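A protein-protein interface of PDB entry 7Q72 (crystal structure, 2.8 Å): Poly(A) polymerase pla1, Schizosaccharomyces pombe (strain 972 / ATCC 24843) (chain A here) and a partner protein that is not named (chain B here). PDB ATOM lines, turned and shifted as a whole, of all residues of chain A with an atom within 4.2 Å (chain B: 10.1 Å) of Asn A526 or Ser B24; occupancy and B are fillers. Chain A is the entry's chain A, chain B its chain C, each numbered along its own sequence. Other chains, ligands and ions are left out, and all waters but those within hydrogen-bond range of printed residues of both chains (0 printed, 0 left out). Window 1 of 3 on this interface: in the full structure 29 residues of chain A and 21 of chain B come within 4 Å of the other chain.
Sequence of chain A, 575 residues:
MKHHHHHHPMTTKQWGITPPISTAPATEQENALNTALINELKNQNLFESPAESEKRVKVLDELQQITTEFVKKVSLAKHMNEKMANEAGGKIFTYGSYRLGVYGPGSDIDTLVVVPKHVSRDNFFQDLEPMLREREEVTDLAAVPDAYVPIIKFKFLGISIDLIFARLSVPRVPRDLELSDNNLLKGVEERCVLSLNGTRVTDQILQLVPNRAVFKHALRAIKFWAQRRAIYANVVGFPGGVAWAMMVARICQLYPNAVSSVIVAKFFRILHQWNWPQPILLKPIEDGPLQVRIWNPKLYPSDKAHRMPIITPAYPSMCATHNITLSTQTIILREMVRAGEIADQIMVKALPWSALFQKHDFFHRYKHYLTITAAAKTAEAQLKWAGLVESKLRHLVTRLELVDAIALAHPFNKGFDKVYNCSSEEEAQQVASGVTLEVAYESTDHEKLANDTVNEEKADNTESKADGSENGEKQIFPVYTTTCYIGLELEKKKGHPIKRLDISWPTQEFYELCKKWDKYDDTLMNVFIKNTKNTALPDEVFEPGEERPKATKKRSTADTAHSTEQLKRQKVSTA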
ATOM      1  N   ALA A 374      20.934  20.501  19.089  1.00  0.00           N
ATOM      2  CA  ALA A 374      20.353  19.238  18.651  1.00  0.00           C
ATOM      3  C   ALA A 374      18.878  19.471  18.370  1.00  0.00           C
ATOM      4  O   ALA A 374      18.141  19.920  19.255  1.00  0.00           O
ATOM      5  CB  ALA A 374      20.537  18.145  19.706  1.00  0.00           C
ATOM      6  N   ALA A 375      18.449  19.169  17.147  1.00  0.00           N
ATOM      7  CA  ALA A 375      17.095  19.456  16.700  1.00  0.00           C
ATOM      8  C   ALA A 375      16.336  18.167  16.414  1.00  0.00           C
ATOM      9  O   ALA A 375      16.930  17.129  16.105  1.00  0.00           O
ATOM     10  CB  ALA A 375      17.103  20.340  15.448  1.00  0.00           C
ATOM     11  N   TRP A 385      16.939  12.691  22.093  1.00  0.00           N
ATOM     12  CA  TRP A 385      18.056  13.145  21.272  1.00  0.00           C
ATOM     13  C   TRP A 385      18.915  14.167  22.008  1.00  0.00           C
ATOM     14  O   TRP A 385      20.141  14.173  21.853  1.00  0.00           O
ATOM     15  CB  TRP A 385      17.529  13.717  19.954  1.00  0.00           C
ATOM     16  CG  TRP A 385      18.586  14.192  19.001  1.00  0.00           C
ATOM     17  CD1 TRP A 385      18.720  15.449  18.491  1.00  0.00           C
ATOM     18  CD2 TRP A 385      19.653  13.415  18.440  1.00  0.00           C
ATOM     19  NE1 TRP A 385      19.804  15.506  17.648  1.00  0.00           N
ATOM     20  CE2 TRP A 385      20.395  14.271  17.601  1.00  0.00           C
ATOM     21  CE3 TRP A 385      20.056  12.083  18.567  1.00  0.00           C
ATOM     22  CZ2 TRP A 385      21.513  13.838  16.894  1.00  0.00           C
ATOM     23  CZ3 TRP A 385      21.168  11.655  17.864  1.00  0.00           C
ATOM     24  CH2 TRP A 385      21.883  12.530  17.038  1.00  0.00           C
ATOM     25  N   ALA A 432      16.810  23.262  10.834  1.00  0.00           N
ATOM     26  CA  ALA A 432      17.533  22.047  11.192  1.00  0.00           C
ATOM     27  C   ALA A 432      19.011  22.114  10.832  1.00  0.00           C
ATOM     28  O   ALA A 432      19.766  21.220  11.227  1.00  0.00           O
ATOM     29  CB  ALA A 432      16.893  20.835  10.515  1.00  0.00           C
ATOM     30  N   SER A 433      19.435  23.134  10.091  1.00  0.00           N
ATOM     31  CA  SER A 433      20.827  23.351   9.736  1.00  0.00           C
ATOM     32  C   SER A 433      21.328  24.637  10.398  1.00  0.00           C
ATOM     33  O   SER A 433      20.638  25.250  11.222  1.00  0.00           O
ATOM     34  CB  SER A 433      20.981  23.388   8.214  1.00  0.00           C
ATOM     35  OG  SER A 433      20.536  22.175   7.629  1.00  0.00           O
ATOM     36  N   ASP A 522      18.077  10.089  10.629  1.00  0.00           N
ATOM     37  CA  ASP A 522      18.213  11.448  10.118  1.00  0.00           C
ATOM     38  C   ASP A 522      16.931  11.975   9.485  1.00  0.00           C
ATOM     39  O   ASP A 522      16.939  13.093   8.961  1.00  0.00           O
ATOM     40  CB  ASP A 522      19.361  11.521   9.107  1.00  0.00           C
ATOM     41  CG  ASP A 522      20.009  12.896   9.061  1.00  0.00           C
ATOM     42  OD1 ASP A 522      19.599  13.780   9.846  1.00  0.00           O
ATOM     43  OD2 ASP A 522      20.932  13.092   8.242  1.00  0.00           O
ATOM     44  N   MET A 525      15.868  13.504  13.460  1.00  0.00           N
ATOM     45  CA  MET A 525      16.825  14.155  14.339  1.00  0.00           C
ATOM     46  C   MET A 525      18.036  14.638  13.552  1.00  0.00           C
ATOM     47  O   MET A 525      18.346  14.135  12.469  1.00  0.00           O
ATOM     48  CB  MET A 525      17.274  13.202  15.455  1.00  0.00           C
ATOM     49  CG  MET A 525      16.125  12.488  16.156  1.00  0.00           C
ATOM     50  SD  MET A 525      16.689  11.179  17.261  1.00  0.00           S
ATOM     51  CE  MET A 525      15.128  10.512  17.825  1.00  0.00           C
ATOM     52  N   ASN A 526      18.723  15.627  14.121  1.00  0.00           N
ATOM     53  CA  ASN A 526      19.937  16.169  13.526  1.00  0.00           C
ATOM     54  C   ASN A 526      20.711  16.911  14.606  1.00  0.00           C
ATOM     55  O   ASN A 526      20.191  17.191  15.690  1.00  0.00           O
ATOM     56  CB  ASN A 526      19.620  17.085  12.341  1.00  0.00           C
ATOM     57  CG  ASN A 526      20.816  17.307  11.440  1.00  0.00           C
ATOM     58  OD1 ASN A 526      21.191  16.432  10.662  1.00  0.00           O
ATOM     59  ND2 ASN A 526      21.420  18.484  11.537  1.00  0.00           N
ATOM     60  N   VAL A 527      21.966  17.226  14.297  1.00  0.00           N
ATOM     61  CA  VAL A 527      22.843  17.937  15.223  1.00  0.00           C
ATOM     62  C   VAL A 527      23.898  18.677  14.412  1.00  0.00           C
ATOM     63  O   VAL A 527      24.452  18.139  13.449  1.00  0.00           O
ATOM     64  CB  VAL A 527      23.484  16.968  16.242  1.00  0.00           C
ATOM     65  CG1 VAL A 527      24.117  15.782  15.532  1.00  0.00           C
ATOM     66  CG2 VAL A 527      24.511  17.690  17.102  1.00  0.00           C
ATOM     67  N   LYS B  20      12.664  12.063   4.113  1.00  0.00           N
ATOM     68  CA  LYS B  20      13.761  12.912   3.682  1.00  0.00           C
ATOM     69  C   LYS B  20      14.680  13.230   4.862  1.00  0.00           C
ATOM     70  O   LYS B  20      14.234  13.278   6.011  1.00  0.00           O
ATOM     71  CB  LYS B  20      13.229  14.205   3.066  1.00  0.00           C
ATOM     72  CG  LYS B  20      12.980  14.134   1.561  1.00  0.00           C
ATOM     73  CD  LYS B  20      11.768  13.280   1.214  1.00  0.00           C
ATOM     74  CE  LYS B  20      10.471  13.956   1.633  1.00  0.00           C
ATOM     75  NZ  LYS B  20       9.280  13.102   1.358  1.00  0.00           N
ATOM     76  N   PRO B  21      15.968  13.443   4.606  1.00  0.00           N
ATOM     77  CA  PRO B  21      16.893  13.743   5.703  1.00  0.00           C
ATOM     78  C   PRO B  21      16.596  15.093   6.336  1.00  0.00           C
ATOM     79  O   PRO B  21      16.187  16.048   5.671  1.00  0.00           O
ATOM     80  CB  PRO B  21      18.268  13.739   5.023  1.00  0.00           C
ATOM     81  CG  PRO B  21      17.979  14.041   3.593  1.00  0.00           C
ATOM     82  CD  PRO B  21      16.659  13.386   3.305  1.00  0.00           C
ATOM     83  N   PHE B  22      16.808  15.158   7.649  1.00  0.00           N
ATOM     84  CA  PHE B  22      16.559  16.365   8.427  1.00  0.00           C
ATOM     85  C   PHE B  22      17.853  17.170   8.491  1.00  0.00           C
ATOM     86  O   PHE B  22      18.799  16.781   9.183  1.00  0.00           O
ATOM     87  CB  PHE B  22      16.057  16.001   9.822  1.00  0.00           C
ATOM     88  CG  PHE B  22      15.255  17.080  10.489  1.00  0.00           C
ATOM     89  CD1 PHE B  22      15.630  17.576  11.727  1.00  0.00           C
ATOM     90  CD2 PHE B  22      14.123  17.595   9.882  1.00  0.00           C
ATOM     91  CE1 PHE B  22      14.889  18.564  12.347  1.00  0.00           C
ATOM     92  CE2 PHE B  22      13.380  18.585  10.496  1.00  0.00           C
ATOM     93  CZ  PHE B  22      13.764  19.071  11.730  1.00  0.00           C
ATOM     94  N   GLY B  23      17.901  18.278   7.754  1.00  0.00           N
ATOM     95  CA  GLY B  23      19.059  19.153   7.753  1.00  0.00           C
ATOM     96  C   GLY B  23      20.321  18.506   7.189  1.00  0.00           C
ATOM     97  O   GLY B  23      20.325  17.390   6.674  1.00  0.00           O
ATOM     98  N   SER B  24      21.411  19.260   7.305  1.00  0.00           N
ATOM     99  CA  SER B  24      22.730  18.804   6.881  1.00  0.00           C
ATOM    100  C   SER B  24      23.766  19.386   7.837  1.00  0.00           C
ATOM    101  O   SER B  24      23.423  20.022   8.839  1.00  0.00           O
ATOM    102  CB  SER B  24      23.001  19.195   5.422  1.00  0.00           C
ATOM    103  OG  SER B  24      23.037  20.604   5.270  1.00  0.00           O
ATOM    104  N   SER B  25      25.043  19.170   7.525  1.00  0.00           N
ATOM    105  CA  SER B  25      26.134  19.629   8.372  1.00  0.00           C
ATOM    106  C   SER B  25      27.221  20.252   7.509  1.00  0.00           C
ATOM    107  O   SER B  25      27.324  19.982   6.310  1.00  0.00           O
ATOM    108  CB  SER B  25      26.714  18.483   9.212  1.00  0.00           C
ATOM    109  OG  SER B  25      25.724  17.901  10.042  1.00  0.00           O
ATOM    110  N   THR B  26      28.037  21.093   8.139  1.00  0.00           N
ATOM    111  CA  THR B  26      29.135  21.787   7.482  1.00  0.00           C
ATOM    112  C   THR B  26      30.326  21.852   8.426  1.00  0.00           C
ATOM    113  O   THR B  26      30.155  21.824   9.650  1.00  0.00           O
ATOM    114  CB  THR B  26      28.743  23.213   7.062  1.00  0.00           C
ATOM    115  OG1 THR B  26      28.111  23.884   8.159  1.00  0.00           O
ATOM    116  CG2 THR B  26      27.802  23.186   5.866  1.00  0.00           C
ATOM    117  N   PRO B  27      31.543  21.927   7.886  1.00  0.00           N
ATOM    118  CA  PRO B  27      32.716  22.109   8.748  1.00  0.00           C
ATOM    119  C   PRO B  27      32.809  23.534   9.270  1.00  0.00           C
ATOM    120  O   PRO B  27      32.430  24.497   8.597  1.00  0.00           O
ATOM    121  CB  PRO B  27      33.891  21.779   7.820  1.00  0.00           C
ATOM    122  CG  PRO B  27      33.380  22.083   6.455  1.00  0.00           C
ATOM    123  CD  PRO B  27      31.920  21.718   6.477  1.00  0.00           C
ATOM    124  N   ASN B  28      33.325  23.660  10.487  1.00  0.00           N
ATOM    125  CA  ASN B  28      33.411  24.941  11.173  1.00  0.00           C
ATOM    126  C   ASN B  28      34.785  25.571  10.984  1.00  0.00           C
ATOM    127  O   ASN B  28      35.767  24.898  10.658  1.00  0.00           O
ATOM    128  CB  ASN B  28      33.120  24.772  12.664  1.00  0.00           C
ATOM    129  CG  ASN B  28      31.790  24.107  12.922  1.00  0.00           C
ATOM    130  OD1 ASN B  28      31.337  23.273  12.139  1.00  0.00           O
ATOM    131  ND2 ASN B  28      31.149  24.477  14.023  1.00  0.00           N
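OG of Ser A433 lies within hydrogen-bond range of N of Ser B24.
The backbone carbonyl oxygen (O) of Asp A522 lies within hydrogen-bond range of the backbone NH (N) of Phe B22.
The side-chain amide oxygen (OD1) of Asn A526 sits close to the backbone carbonyl oxygen (O) of Phe B22, at 2.8 Å.
O of Asn A526 sits at hydrogen-bond distance from N of Ala A375.
O of Asn A526 lies within hydrogen-bond range of NE1 of Trp A385, at 2.6 Å.
O of Ala A432 is in hydrogen-bond range of ND2 of Asn A526 (3.2 Å).
The side-chain amide oxygen of Asn A526 sits close to the side-chain carboxylate of Asp A522 (3.2 Å).
CE1 of Phe B22 touches CB of Ala A432, 3.5 Å away.
Ala A432 touches Gly B23.
OG of Ser A433 touches CA of Gly B23, at 3.4 Å.
O of Asp A522 touches C of Pro B21, 3.3 Å away.
CB of Phe B22 touches O of Met A525, at 3.97 Å.
Asn A526 touches Ser B24.
O of Val A527 touches OG of Ser B25 (3.6 Å).
Printed residues of chain B within 4 Å of Ala A432: Phe B22 and Gly B23.
Of the printed residues of chain B, Asp A522 touches Pro B21 and Phe B22.
Of the printed residues of chain B, Met A525 touches Phe B22 (3.97 Å).
Printed residues of chain B within 4 Å of Asn A526: Phe B22 (2.8 Å) and Ser B24 (3.7 Å).
Val A527 touches just one residue of chain B: Ser B25 (3.6 Å).
Printed residues of chain A within 4 Å of Pro B21: Asp A522.
Ser B24 touches just these residues of chain A: Ser A433 and Asn A526.
Of the printed residues of chain A, Ser B25 touches Val A527 (3.6 Å).
Thr B26 touches none of the printed residues of chain A.
The nearest residue of chain B that does not touch Asn A526 is Gly B23 (4.1 Å).
The nearest printed residue of chain A that does not touch Ser B24 is Ala A432 (4.5 Å).
Of the 9 printed residues of chain B, 5 touch a printed residue of chain A.
Of the 9 printed residues of chain A, 6 touch a printed residue of chain B.
Printed residues of chain A that touch a printed residue of chain B: Ala A432, Ser A433, Asp A522, Met A525, Asn A526 and Val A527.
Among the printed residues, no Asp or Glu carboxylate lies within 4 Å of a Lys or Arg side-chain nitrogen of the other chain.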
